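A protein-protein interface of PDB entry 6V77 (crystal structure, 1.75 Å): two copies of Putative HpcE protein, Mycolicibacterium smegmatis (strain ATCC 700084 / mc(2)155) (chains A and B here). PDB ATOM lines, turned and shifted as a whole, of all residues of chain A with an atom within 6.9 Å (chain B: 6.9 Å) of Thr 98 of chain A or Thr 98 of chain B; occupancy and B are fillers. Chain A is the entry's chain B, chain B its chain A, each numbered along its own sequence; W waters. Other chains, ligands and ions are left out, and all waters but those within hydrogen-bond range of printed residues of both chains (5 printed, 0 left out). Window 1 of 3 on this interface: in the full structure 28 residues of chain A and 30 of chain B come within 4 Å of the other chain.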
ATOM      1  N   GLN A  71       5.226 -30.024 -15.996  1.00  0.00           N
ATOM      2  CA  GLN A  71       5.509 -28.791 -16.713  1.00  0.00           C
ATOM      3  C   GLN A  71       4.514 -28.686 -17.852  1.00  0.00           C
ATOM      4  O   GLN A  71       4.218 -29.695 -18.497  1.00  0.00           O
ATOM      5  CB  GLN A  71       6.936 -28.778 -17.281  1.00  0.00           C
ATOM      6  CG  GLN A  71       7.994 -28.875 -16.180  1.00  0.00           C
ATOM      7  CD  GLN A  71       9.414 -29.034 -16.716  1.00  0.00           C
ATOM      8  OE1 GLN A  71      10.331 -28.331 -16.265  1.00  0.00           O
ATOM      9  NE2 GLN A  71       9.608 -29.949 -17.672  1.00  0.00           N
ATOM     10  N   VAL A  72       4.004 -27.475 -18.081  1.00  0.00           N
ATOM     11  CA  VAL A  72       3.105 -27.175 -19.202  1.00  0.00           C
ATOM     12  C   VAL A  72       3.777 -26.106 -20.039  1.00  0.00           C
ATOM     13  O   VAL A  72       4.057 -25.004 -19.539  1.00  0.00           O
ATOM     14  CB  VAL A  72       1.739 -26.667 -18.721  1.00  0.00           C
ATOM     15  CG1 VAL A  72       0.869 -26.261 -19.925  1.00  0.00           C
ATOM     16  CG2 VAL A  72       1.049 -27.700 -17.841  1.00  0.00           C
ATOM     17  N   PHE A  73       3.983 -26.393 -21.308  1.00  0.00           N
ATOM     18  CA  PHE A  73       4.569 -25.424 -22.223  1.00  0.00           C
ATOM     19  C   PHE A  73       3.500 -24.958 -23.187  1.00  0.00           C
ATOM     20  O   PHE A  73       2.912 -25.772 -23.902  1.00  0.00           O
ATOM     21  CB  PHE A  73       5.736 -26.046 -22.977  1.00  0.00           C
ATOM     22  CG  PHE A  73       6.771 -26.565 -22.058  1.00  0.00           C
ATOM     23  CD1 PHE A  73       7.695 -25.708 -21.490  1.00  0.00           C
ATOM     24  CD2 PHE A  73       6.763 -27.902 -21.681  1.00  0.00           C
ATOM     25  CE1 PHE A  73       8.663 -26.169 -20.592  1.00  0.00           C
ATOM     26  CE2 PHE A  73       7.750 -28.391 -20.784  1.00  0.00           C
ATOM     27  CZ  PHE A  73       8.678 -27.515 -20.223  1.00  0.00           C
ATOM     28  N   ALA A  74       3.262 -23.661 -23.223  1.00  0.00           N
ATOM     29  CA  ALA A  74       2.283 -23.117 -24.163  1.00  0.00           C
ATOM     30  C   ALA A  74       3.018 -22.213 -25.136  1.00  0.00           C
ATOM     31  O   ALA A  74       3.842 -21.390 -24.723  1.00  0.00           O
ATOM     32  CB  ALA A  74       1.178 -22.366 -23.430  1.00  0.00           C
ATOM     33  N   VAL A  75       2.725 -22.371 -26.420  1.00  0.00           N
ATOM     34  CA  VAL A  75       3.475 -21.737 -27.491  1.00  0.00           C
ATOM     35  C   VAL A  75       2.606 -20.636 -28.083  1.00  0.00           C
ATOM     36  O   VAL A  75       1.437 -20.873 -28.408  1.00  0.00           O
ATOM     37  CB  VAL A  75       3.876 -22.769 -28.554  1.00  0.00           C
ATOM     38  CG1 VAL A  75       4.623 -22.107 -29.701  1.00  0.00           C
ATOM     39  CG2 VAL A  75       4.721 -23.899 -27.901  1.00  0.00           C
ATOM     40  N   ILE A  96       7.383 -18.916 -25.609  1.00  0.00           N
ATOM     41  CA  ILE A  96       7.021 -19.948 -24.639  1.00  0.00           C
ATOM     42  C   ILE A  96       6.469 -19.308 -23.366  1.00  0.00           C
ATOM     43  O   ILE A  96       7.111 -18.435 -22.765  1.00  0.00           O
ATOM     44  CB  ILE A  96       8.217 -20.865 -24.308  1.00  0.00           C
ATOM     45  CG1 ILE A  96       8.758 -21.540 -25.591  1.00  0.00           C
ATOM     46  CG2 ILE A  96       7.807 -21.878 -23.242  1.00  0.00           C
ATOM     47  CD1 ILE A  96       7.757 -22.451 -26.321  1.00  0.00           C
ATOM     48  N   PHE A  97       5.301 -19.780 -22.935  1.00  0.00           N
ATOM     49  CA  PHE A  97       4.740 -19.407 -21.642  1.00  0.00           C
ATOM     50  C   PHE A  97       4.096 -20.658 -21.055  1.00  0.00           C
ATOM     51  O   PHE A  97       4.357 -21.781 -21.495  1.00  0.00           O
ATOM     52  CB  PHE A  97       3.767 -18.221 -21.764  1.00  0.00           C
ATOM     53  CG  PHE A  97       2.795 -18.355 -22.884  1.00  0.00           C
ATOM     54  CD1 PHE A  97       1.568 -18.952 -22.677  1.00  0.00           C
ATOM     55  CD2 PHE A  97       3.100 -17.878 -24.147  1.00  0.00           C
ATOM     56  CE1 PHE A  97       0.659 -19.081 -23.728  1.00  0.00           C
ATOM     57  CE2 PHE A  97       2.197 -18.016 -25.202  1.00  0.00           C
ATOM     58  CZ  PHE A  97       0.985 -18.613 -24.993  1.00  0.00           C
ATOM     59  N   THR A  98       3.283 -20.497 -20.021  1.00  0.00           N
ATOM     60  CA  THR A  98       2.691 -21.686 -19.425  1.00  0.00           C
ATOM     61  C   THR A  98       1.194 -21.463 -19.255  1.00  0.00           C
ATOM     62  O   THR A  98       0.681 -20.352 -19.406  1.00  0.00           O
ATOM     63  CB  THR A  98       3.360 -22.052 -18.078  1.00  0.00           C
ATOM     64  OG1 THR A  98       2.993 -23.396 -17.717  1.00  0.00           O
ATOM     65  CG2 THR A  98       2.936 -21.071 -16.966  1.00  0.00           C
ATOM     66  N   LYS A  99       0.489 -22.554 -19.001  1.00  0.00           N
ATOM     67  CA  LYS A  99      -0.903 -22.515 -18.573  1.00  0.00           C
ATOM     68  C   LYS A  99      -0.931 -23.304 -17.272  1.00  0.00           C
ATOM     69  O   LYS A  99      -0.628 -24.504 -17.270  1.00  0.00           O
ATOM     70  CB  LYS A  99      -1.823 -23.096 -19.653  1.00  0.00           C
ATOM     71  CG  LYS A  99      -1.968 -22.155 -20.866  1.00  0.00           C
ATOM     72  CD  LYS A  99      -2.472 -22.857 -22.150  1.00  0.00           C
ATOM     73  CE  LYS A  99      -3.941 -23.234 -22.066  1.00  0.00           C
ATOM     74  NZ  LYS A  99      -4.843 -22.079 -21.793  1.00  0.00           N
ATOM     75  N   PHE A 100      -1.214 -22.620 -16.163  1.00  0.00           N
ATOM     76  CA  PHE A 100      -1.007 -23.245 -14.856  1.00  0.00           C
ATOM     77  C   PHE A 100      -1.924 -24.451 -14.685  1.00  0.00           C
ATOM     78  O   PHE A 100      -3.045 -24.471 -15.200  1.00  0.00           O
ATOM     79  CB  PHE A 100      -1.215 -22.212 -13.746  1.00  0.00           C
ATOM     80  CG  PHE A 100      -0.133 -21.151 -13.716  1.00  0.00           C
ATOM     81  CD1 PHE A 100       1.158 -21.484 -13.274  1.00  0.00           C
ATOM     82  CD2 PHE A 100      -0.367 -19.868 -14.179  1.00  0.00           C
ATOM     83  CE1 PHE A 100       2.165 -20.536 -13.260  1.00  0.00           C
ATOM     84  CE2 PHE A 100       0.640 -18.908 -14.165  1.00  0.00           C
ATOM     85  CZ  PHE A 100       1.912 -19.250 -13.705  1.00  0.00           C
ATOM     86  N   VAL A 101      -1.414 -25.484 -14.000  1.00  0.00           N
ATOM     87  CA  VAL A 101      -2.091 -26.778 -13.993  1.00  0.00           C
ATOM     88  C   VAL A 101      -3.488 -26.720 -13.372  1.00  0.00           C
ATOM     89  O   VAL A 101      -4.354 -27.521 -13.742  1.00  0.00           O
ATOM     90  CB  VAL A 101      -1.197 -27.846 -13.301  1.00  0.00           C
ATOM     91  CG1 VAL A 101      -1.205 -27.723 -11.777  1.00  0.00           C
ATOM     92  CG2 VAL A 101      -1.595 -29.241 -13.739  1.00  0.00           C
ATOM     93  N   ASP A 152      -6.659 -23.153 -25.972  1.00  0.00           N
ATOM     94  CA  ASP A 152      -5.933 -22.184 -25.147  1.00  0.00           C
ATOM     95  C   ASP A 152      -6.823 -20.954 -24.991  1.00  0.00           C
ATOM     96  O   ASP A 152      -6.635 -19.928 -25.644  1.00  0.00           O
ATOM     97  CB  ASP A 152      -4.581 -21.829 -25.760  1.00  0.00           C
ATOM     98  CG  ASP A 152      -3.813 -20.828 -24.925  1.00  0.00           C
ATOM     99  OD1 ASP A 152      -4.201 -20.583 -23.758  1.00  0.00           O
ATOM    100  OD2 ASP A 152      -2.805 -20.284 -25.406  1.00  0.00           O
ATOM    101  N   GLN A 166       2.913 -10.486 -19.692  1.00  0.00           N
ATOM    102  CA  GLN A 166       3.186 -11.916 -19.614  1.00  0.00           C
ATOM    103  C   GLN A 166       1.871 -12.689 -19.715  1.00  0.00           C
ATOM    104  O   GLN A 166       0.922 -12.399 -18.980  1.00  0.00           O
ATOM    105  CB  GLN A 166       3.914 -12.234 -18.308  1.00  0.00           C
ATOM    106  CG  GLN A 166       5.177 -11.410 -18.129  1.00  0.00           C
ATOM    107  CD  GLN A 166       6.250 -11.779 -19.143  1.00  0.00           C
ATOM    108  OE1 GLN A 166       6.660 -12.934 -19.241  1.00  0.00           O
ATOM    109  NE2 GLN A 166       6.703 -10.796 -19.901  1.00  0.00           N
ATOM    110  N   PHE A 167       1.832 -13.691 -20.595  1.00  0.00           N
ATOM    111  CA  PHE A 167       0.579 -14.255 -21.083  1.00  0.00           C
ATOM    112  C   PHE A 167      -0.035 -15.341 -20.197  1.00  0.00           C
ATOM    113  O   PHE A 167      -1.215 -15.657 -20.381  1.00  0.00           O
ATOM    114  CB  PHE A 167       0.776 -14.833 -22.492  1.00  0.00           C
ATOM    115  CG  PHE A 167       1.182 -13.809 -23.537  1.00  0.00           C
ATOM    116  CD1 PHE A 167       1.102 -12.449 -23.276  1.00  0.00           C
ATOM    117  CD2 PHE A 167       1.615 -14.221 -24.795  1.00  0.00           C
ATOM    118  CE1 PHE A 167       1.459 -11.509 -24.240  1.00  0.00           C
ATOM    119  CE2 PHE A 167       1.962 -13.272 -25.773  1.00  0.00           C
ATOM    120  CZ  PHE A 167       1.886 -11.927 -25.489  1.00  0.00           C
ATOM    121  N   SER A 168       0.703 -15.911 -19.239  1.00  0.00           N
ATOM    122  CA  SER A 168       0.263 -17.170 -18.637  1.00  0.00           C
ATOM    123  C   SER A 168      -1.028 -17.008 -17.838  1.00  0.00           C
ATOM    124  O   SER A 168      -1.932 -17.839 -17.943  1.00  0.00           O
ATOM    125  CB  SER A 168       1.360 -17.740 -17.729  1.00  0.00           C
ATOM    126  OG  SER A 168       2.529 -17.994 -18.477  1.00  0.00           O
ATOM    127  N   LEU A 169      -1.102 -15.988 -16.991  1.00  0.00           N
ATOM    128  CA  LEU A 169      -2.212 -15.896 -16.048  1.00  0.00           C
ATOM    129  C   LEU A 169      -3.543 -15.732 -16.775  1.00  0.00           C
ATOM    130  O   LEU A 169      -4.532 -16.387 -16.424  1.00  0.00           O
ATOM    131  CB  LEU A 169      -1.981 -14.732 -15.079  1.00  0.00           C
ATOM    132  CG  LEU A 169      -2.645 -14.884 -13.714  1.00  0.00           C
ATOM    133  CD1 LEU A 169      -2.140 -16.121 -12.983  1.00  0.00           C
ATOM    134  CD2 LEU A 169      -2.460 -13.612 -12.865  1.00  0.00           C
ATOM    135  N   LYS A 171      -4.391 -16.950 -19.469  1.00  0.00           N
ATOM    136  CA  LYS A 171      -4.714 -18.227 -20.080  1.00  0.00           C
ATOM    137  C   LYS A 171      -4.891 -19.328 -19.047  1.00  0.00           C
ATOM    138  O   LYS A 171      -4.940 -20.501 -19.416  1.00  0.00           O
ATOM    139  CB  LYS A 171      -3.633 -18.598 -21.088  1.00  0.00           C
ATOM    140  CG  LYS A 171      -3.548 -17.577 -22.243  1.00  0.00           C
ATOM    141  CD  LYS A 171      -2.216 -17.733 -22.962  1.00  0.00           C
ATOM    142  CE  LYS A 171      -2.142 -16.913 -24.233  1.00  0.00           C
ATOM    143  NZ  LYS A 171      -3.006 -17.508 -25.314  1.00  0.00           N
ATOM    144  N   SER A 172      -5.046 -18.960 -17.762  1.00  0.00           N
ATOM    145  CA  SER A 172      -5.083 -19.938 -16.679  1.00  0.00           C
ATOM    146  C   SER A 172      -6.272 -19.736 -15.754  1.00  0.00           C
ATOM    147  O   SER A 172      -6.244 -20.195 -14.607  1.00  0.00           O
ATOM    148  CB  SER A 172      -3.780 -19.902 -15.865  1.00  0.00           C
ATOM    149  OG  SER A 172      -2.691 -20.192 -16.710  1.00  0.00           O
ATOM    150  N   GLN B  71       2.591 -25.705  -9.079  1.00  0.00           N
ATOM    151  CA  GLN B  71       2.590 -24.429  -9.780  1.00  0.00           C
ATOM    152  C   GLN B  71       3.708 -23.557  -9.215  1.00  0.00           C
ATOM    153  O   GLN B  71       3.892 -23.486  -7.993  1.00  0.00           O
ATOM    154  CB  GLN B  71       1.216 -23.696  -9.624  1.00  0.00           C
ATOM    155  CG  GLN B  71       0.046 -24.521 -10.177  1.00  0.00           C
ATOM    156  CD  GLN B  71      -1.329 -23.898  -9.942  1.00  0.00           C
ATOM    157  OE1 GLN B  71      -2.166 -23.860 -10.853  1.00  0.00           O
ATOM    158  NE2 GLN B  71      -1.586 -23.455  -8.702  1.00  0.00           N
ATOM    159  N   VAL B  72       4.436 -22.877 -10.102  1.00  0.00           N
ATOM    160  CA  VAL B  72       5.488 -21.930  -9.712  1.00  0.00           C
ATOM    161  C   VAL B  72       5.126 -20.564 -10.281  1.00  0.00           C
ATOM    162  O   VAL B  72       4.974 -20.422 -11.498  1.00  0.00           O
ATOM    163  CB  VAL B  72       6.869 -22.353 -10.237  1.00  0.00           C
ATOM    164  CG1 VAL B  72       7.909 -21.278  -9.859  1.00  0.00           C
ATOM    165  CG2 VAL B  72       7.258 -23.711  -9.698  1.00  0.00           C
ATOM    166  N   PHE B  73       5.040 -19.560  -9.414  1.00  0.00           N
ATOM    167  CA  PHE B  73       4.720 -18.199  -9.817  1.00  0.00           C
ATOM    168  C   PHE B  73       5.946 -17.346  -9.551  1.00  0.00           C
ATOM    169  O   PHE B  73       6.514 -17.401  -8.457  1.00  0.00           O
ATOM    170  CB  PHE B  73       3.506 -17.680  -9.048  1.00  0.00           C
ATOM    171  CG  PHE B  73       2.319 -18.586  -9.149  1.00  0.00           C
ATOM    172  CD1 PHE B  73       1.459 -18.509 -10.238  1.00  0.00           C
ATOM    173  CD2 PHE B  73       2.102 -19.555  -8.183  1.00  0.00           C
ATOM    174  CE1 PHE B  73       0.374 -19.372 -10.349  1.00  0.00           C
ATOM    175  CE2 PHE B  73       1.041 -20.426  -8.286  1.00  0.00           C
ATOM    176  CZ  PHE B  73       0.163 -20.332  -9.359  1.00  0.00           C
ATOM    177  N   ALA B  74       6.386 -16.617 -10.559  1.00  0.00           N
ATOM    178  CA  ALA B  74       7.509 -15.711 -10.403  1.00  0.00           C
ATOM    179  C   ALA B  74       7.059 -14.318 -10.806  1.00  0.00           C
ATOM    180  O   ALA B  74       6.301 -14.153 -11.765  1.00  0.00           O
ATOM    181  CB  ALA B  74       8.722 -16.175 -11.225  1.00  0.00           C
ATOM    182  N   VAL B  75       7.498 -13.321 -10.049  1.00  0.00           N
ATOM    183  CA  VAL B  75       6.976 -11.968 -10.179  1.00  0.00           C
ATOM    184  C   VAL B  75       8.062 -11.081 -10.762  1.00  0.00           C
ATOM    185  O   VAL B  75       9.232 -11.183 -10.377  1.00  0.00           O
ATOM    186  CB  VAL B  75       6.498 -11.431  -8.816  1.00  0.00           C
ATOM    187  CG1 VAL B  75       5.880 -10.041  -8.976  1.00  0.00           C
ATOM    188  CG2 VAL B  75       5.501 -12.392  -8.200  1.00  0.00           C
ATOM    189  N   ILE B  96       3.323 -11.654 -13.904  1.00  0.00           N
ATOM    190  CA  ILE B  96       3.476 -13.040 -13.458  1.00  0.00           C
ATOM    191  C   ILE B  96       3.963 -13.924 -14.604  1.00  0.00           C
ATOM    192  O   ILE B  96       3.364 -13.943 -15.688  1.00  0.00           O
ATOM    193  CB  ILE B  96       2.149 -13.588 -12.893  1.00  0.00           C
ATOM    194  CG1 ILE B  96       1.698 -12.752 -11.688  1.00  0.00           C
ATOM    195  CG2 ILE B  96       2.281 -15.072 -12.556  1.00  0.00           C
ATOM    196  CD1 ILE B  96       2.717 -12.682 -10.582  1.00  0.00           C
ATOM    197  N   PHE B  97       5.000 -14.718 -14.331  1.00  0.00           N
ATOM    198  CA  PHE B  97       5.451 -15.760 -15.243  1.00  0.00           C
ATOM    199  C   PHE B  97       5.790 -16.992 -14.396  1.00  0.00           C
ATOM    200  O   PHE B  97       5.391 -17.084 -13.234  1.00  0.00           O
ATOM    201  CB  PHE B  97       6.624 -15.253 -16.091  1.00  0.00           C
ATOM    202  CG  PHE B  97       7.677 -14.534 -15.285  1.00  0.00           C
ATOM    203  CD1 PHE B  97       7.572 -13.175 -15.055  1.00  0.00           C
ATOM    204  CD2 PHE B  97       8.759 -15.223 -14.754  1.00  0.00           C
ATOM    205  CE1 PHE B  97       8.519 -12.502 -14.307  1.00  0.00           C
ATOM    206  CE2 PHE B  97       9.717 -14.552 -14.008  1.00  0.00           C
ATOM    207  CZ  PHE B  97       9.599 -13.193 -13.786  1.00  0.00           C
ATOM    208  N   THR B  98       6.495 -17.973 -14.969  1.00  0.00           N
ATOM    209  CA  THR B  98       6.862 -19.164 -14.203  1.00  0.00           C
ATOM    210  C   THR B  98       8.360 -19.442 -14.328  1.00  0.00           C
ATOM    211  O   THR B  98       9.073 -18.838 -15.131  1.00  0.00           O
ATOM    212  CB  THR B  98       6.047 -20.412 -14.636  1.00  0.00           C
ATOM    213  OG1 THR B  98       6.128 -21.437 -13.619  1.00  0.00           O
ATOM    214  CG2 THR B  98       6.558 -20.980 -15.975  1.00  0.00           C
ATOM    215  N   LYS B  99       8.836 -20.336 -13.475  1.00  0.00           N
ATOM    216  CA  LYS B  99      10.161 -20.921 -13.606  1.00  0.00           C
ATOM    217  C   LYS B  99       9.915 -22.422 -13.594  1.00  0.00           C
ATOM    218  O   LYS B  99       9.391 -22.955 -12.613  1.00  0.00           O
ATOM    219  CB  LYS B  99      11.096 -20.448 -12.476  1.00  0.00           C
ATOM    220  CG  LYS B  99      11.453 -18.954 -12.623  1.00  0.00           C
ATOM    221  CD  LYS B  99      11.931 -18.269 -11.337  1.00  0.00           C
ATOM    222  CE  LYS B  99      13.258 -18.890 -10.806  1.00  0.00           C
ATOM    223  NZ  LYS B  99      14.363 -18.755 -11.827  1.00  0.00           N
ATOM    224  N   PHE B 100      10.218 -23.088 -14.707  1.00  0.00           N
ATOM    225  CA  PHE B 100       9.780 -24.467 -14.859  1.00  0.00           C
ATOM    226  C   PHE B 100      10.452 -25.364 -13.819  1.00  0.00           C
ATOM    227  O   PHE B 100      11.597 -25.138 -13.416  1.00  0.00           O
ATOM    228  CB  PHE B 100      10.052 -24.944 -16.277  1.00  0.00           C
ATOM    229  CG  PHE B 100       9.187 -24.259 -17.285  1.00  0.00           C
ATOM    230  CD1 PHE B 100       7.836 -24.569 -17.359  1.00  0.00           C
ATOM    231  CD2 PHE B 100       9.706 -23.294 -18.134  1.00  0.00           C
ATOM    232  CE1 PHE B 100       6.995 -23.930 -18.295  1.00  0.00           C
ATOM    233  CE2 PHE B 100       8.878 -22.655 -19.076  1.00  0.00           C
ATOM    234  CZ  PHE B 100       7.530 -22.980 -19.155  1.00  0.00           C
ATOM    235  N   VAL B 101       9.709 -26.375 -13.357  1.00  0.00           N
ATOM    236  CA  VAL B 101      10.124 -27.067 -12.136  1.00  0.00           C
ATOM    237  C   VAL B 101      11.430 -27.825 -12.345  1.00  0.00           C
ATOM    238  O   VAL B 101      12.182 -28.016 -11.383  1.00  0.00           O
ATOM    239  CB  VAL B 101       8.981 -27.969 -11.609  1.00  0.00           C
ATOM    240  CG1 VAL B 101       8.726 -29.178 -12.512  1.00  0.00           C
ATOM    241  CG2 VAL B 101       9.222 -28.366 -10.148  1.00  0.00           C
ATOM    242  N   ASP B 152      16.523 -15.896  -8.689  1.00  0.00           N
ATOM    243  CA  ASP B 152      15.867 -15.980  -9.999  1.00  0.00           C
ATOM    244  C   ASP B 152      16.907 -15.691 -11.078  1.00  0.00           C
ATOM    245  O   ASP B 152      16.941 -14.622 -11.681  1.00  0.00           O
ATOM    246  CB  ASP B 152      14.674 -15.023 -10.075  1.00  0.00           C
ATOM    247  CG  ASP B 152      13.918 -15.125 -11.405  1.00  0.00           C
ATOM    248  OD1 ASP B 152      14.238 -16.030 -12.208  1.00  0.00           O
ATOM    249  OD2 ASP B 152      12.995 -14.305 -11.673  1.00  0.00           O
ATOM    250  N   GLN B 166       8.439 -13.240 -23.470  1.00  0.00           N
ATOM    251  CA  GLN B 166       7.894 -14.029 -22.377  1.00  0.00           C
ATOM    252  C   GLN B 166       9.064 -14.578 -21.572  1.00  0.00           C
ATOM    253  O   GLN B 166       9.954 -15.217 -22.138  1.00  0.00           O
ATOM    254  CB  GLN B 166       7.025 -15.166 -22.930  1.00  0.00           C
ATOM    255  CG  GLN B 166       5.860 -14.647 -23.786  1.00  0.00           C
ATOM    256  CD  GLN B 166       4.905 -13.787 -22.996  1.00  0.00           C
ATOM    257  OE1 GLN B 166       4.308 -14.241 -22.018  1.00  0.00           O
ATOM    258  NE2 GLN B 166       4.753 -12.535 -23.411  1.00  0.00           N
ATOM    259  N   PHE B 167       9.054 -14.342 -20.258  1.00  0.00           N
ATOM    260  CA  PHE B 167      10.279 -14.439 -19.460  1.00  0.00           C
ATOM    261  C   PHE B 167      10.630 -15.842 -18.958  1.00  0.00           C
ATOM    262  O   PHE B 167      11.745 -16.019 -18.465  1.00  0.00           O
ATOM    263  CB  PHE B 167      10.189 -13.518 -18.231  1.00  0.00           C
ATOM    264  CG  PHE B 167      10.055 -12.044 -18.559  1.00  0.00           C
ATOM    265  CD1 PHE B 167      10.364 -11.558 -19.814  1.00  0.00           C
ATOM    266  CD2 PHE B 167       9.661 -11.147 -17.574  1.00  0.00           C
ATOM    267  CE1 PHE B 167      10.253 -10.204 -20.110  1.00  0.00           C
ATOM    268  CE2 PHE B 167       9.551  -9.787 -17.860  1.00  0.00           C
ATOM    269  CZ  PHE B 167       9.845  -9.317 -19.133  1.00  0.00           C
ATOM    270  N   SER B 168       9.744 -16.845 -19.049  1.00  0.00           N
ATOM    271  CA  SER B 168       9.946 -18.049 -18.225  1.00  0.00           C
ATOM    272  C   SER B 168      11.149 -18.874 -18.672  1.00  0.00           C
ATOM    273  O   SER B 168      11.930 -19.346 -17.834  1.00  0.00           O
ATOM    274  CB  SER B 168       8.695 -18.929 -18.243  1.00  0.00           C
ATOM    275  OG  SER B 168       7.581 -18.209 -17.721  1.00  0.00           O
ATOM    276  N   LEU B 169      11.290 -19.115 -19.978  1.00  0.00           N
ATOM    277  CA  LEU B 169      12.316 -20.065 -20.417  1.00  0.00           C
ATOM    278  C   LEU B 169      13.717 -19.589 -20.043  1.00  0.00           C
ATOM    279  O   LEU B 169      14.566 -20.385 -19.602  1.00  0.00           O
ATOM    280  CB  LEU B 169      12.212 -20.286 -21.926  1.00  0.00           C
ATOM    281  CG  LEU B 169      12.850 -21.575 -22.466  1.00  0.00           C
ATOM    282  CD1 LEU B 169      12.192 -22.821 -21.862  1.00  0.00           C
ATOM    283  CD2 LEU B 169      12.724 -21.608 -23.986  1.00  0.00           C
ATOM    284  N   LYS B 171      14.639 -18.037 -17.538  1.00  0.00           N
ATOM    285  CA  LYS B 171      14.829 -18.197 -16.105  1.00  0.00           C
ATOM    286  C   LYS B 171      14.694 -19.651 -15.679  1.00  0.00           C
ATOM    287  O   LYS B 171      14.504 -19.933 -14.490  1.00  0.00           O
ATOM    288  CB  LYS B 171      13.814 -17.320 -15.366  1.00  0.00           C
ATOM    289  CG  LYS B 171      13.915 -15.847 -15.761  1.00  0.00           C
ATOM    290  CD  LYS B 171      12.724 -15.030 -15.251  1.00  0.00           C
ATOM    291  CE  LYS B 171      12.995 -13.530 -15.325  1.00  0.00           C
ATOM    292  NZ  LYS B 171      13.820 -13.049 -14.165  1.00  0.00           N
ATOM    293  N   SER B 172      14.773 -20.582 -16.634  1.00  0.00           N
ATOM    294  CA  SER B 172      14.498 -21.982 -16.339  1.00  0.00           C
ATOM    295  C   SER B 172      15.618 -22.894 -16.834  1.00  0.00           C
ATOM    296  O   SER B 172      15.397 -24.100 -16.993  1.00  0.00           O
ATOM    297  CB  SER B 172      13.154 -22.423 -16.931  1.00  0.00           C
ATOM    298  OG  SER B 172      12.075 -21.647 -16.381  1.00  0.00           O
HETATM  299  O   HOH W   1       5.175 -15.062 -19.779  1.00  0.00           O
HETATM  300  O   HOH W   2       3.425 -15.570 -18.101  1.00  0.00           O
HETATM  301  O   HOH W   3       0.809 -13.813 -16.467  1.00  0.00           O
HETATM  302  O   HOH W   4       6.971 -17.064 -20.099  1.00  0.00           O
HETATM  303  O   HOH W   5       9.726 -18.066 -22.217  1.00  0.00           O
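Val 72 of chain A touches Phe 100 of chain B, and with the chains exchanged Phe 100 of chain A touches Val 72 of chain B.
Thr 98 of chain A touches its own counterpart, Thr 98 of chain B.
Gln 166 of chain A touches Phe 97 of chain B, but with the chains exchanged Phe 97 of chain A does not touch Gln 166 of chain B (4.02 Å).
Gln 166 of chain A touches Phe 167 of chain B, and with the chains exchanged Phe 167 of chain A touches Gln 166 of chain B.
Positions printed for both chains: 71, 72, 73, 74, 75, 96, 97, 98, 99, 100, 101, 152, 166, 167, 168, 169, 171 and 172.
Of the 18 printed residues of chain A, 9 touch a printed residue of chain B.
Among the printed residues, 15 pairs touch across the chains.
Among the printed residues, no Asp or Glu carboxylate lies within 4 Å of a Lys or Arg side-chain nitrogen of the other chain.
Water W2 bridges OG of Ser 168 of chain A (2.6 Å) and O of Ile 96 of chain B (2.9 Å).
Water W3 lies within hydrogen-bond range of O of Ile 96 of chain B, O of Gln 166 of chain A, N of Leu 169 of chain A and N of Ser 168 of chain A.
Water W5 lies within hydrogen-bond range of O of Ile 96 of chain A, O of Gln 166 of chain B, N of Leu 169 of chain B and N of Ser 168 of chain B.
Water W4 lies within hydrogen-bond range of the side-chain hydroxyl (OG) of Ser 168 of chain B (2.7 Å), the backbone carbonyl oxygen (O) of Ile 96 of chain A (3.0 Å) and the backbone NH (N) of Phe 167 of chain B (3.4 Å).
N of Phe 167 of chain A sits at hydrogen-bond distance from OE1 of Gln 166 of chain B.
The backbone NH (N) of Phe 167 of chain B sits at hydrogen-bond distance from the side-chain amide oxygen (OE1) of Gln 166 of chain A.
Gln 71 of chain A touches Phe 100 of chain B.
N of Val 101 of chain B touches OE1 of Gln 71 of chain A (3.6 Å).
Phe 100 of chain B touches Val 72 of chain A.
Phe 73 of chain A touches Phe 100 of chain B (CD1 to CZ, 3.6 Å).
Ile 96 of chain A touches Gln 166 of chain B.
CG2 of Thr 98 of chain A touches CG2 of Thr 98 of chain B, at 3.8 Å.
Phe 100 of chain A touches Gln 71 of chain B.
Val 72 of chain B touches Phe 100 of chain A.
OE1 of Gln 71 of chain B touches N of Val 101 of chain A, 3.6 Å away.
CB of Gln 166 of chain A touches O of Ile 96 of chain B, at 3.2 Å.
Thr 98 of chain A touches just one residue of chain B: Thr 98.
Thr 98 of chain B touches one residue of chain A.
Of the printed residues of chain B, Phe 100 of chain A touches Gln 71 (3.5 Å), Val 72 (3.3 Å) and Phe 73 (3.6 Å).
Of the printed residues of chain B, Val 72 of chain A touches Phe 100 (3.4 Å).
Lys 171 of chain B touches none of the printed residues of chain A.
The nearest residue of chain B that does not touch Thr 98 of chain A is Phe 100 of chain B (4.1 Å).
The backbone NH (N) of Ala 74 of chain B is in hydrogen-bond range of the backbone carbonyl oxygen (O) of Phe 97 of chain B (2.9 Å).
The side-chain hydroxyl of Thr 98 of chain B sits at hydrogen-bond distance from the backbone carbonyl oxygen of Val 72 of chain B, at 2.6 Å.
The backbone NH (N) of Thr 98 of chain A is in hydrogen-bond range of the side-chain hydroxyl (OG) of Ser 168 of chain A.
OG1 of Thr 98 of chain A is in hydrogen-bond range of O of Val 72 of chain A (2.7 Å).
N of Thr 98 of chain B is in hydrogen-bond range of OG of Ser 168 of chain B, 3.0 Å away.
N of Phe 100 of chain B is in hydrogen-bond range of OG of Ser 172 of chain B (2.9 Å).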
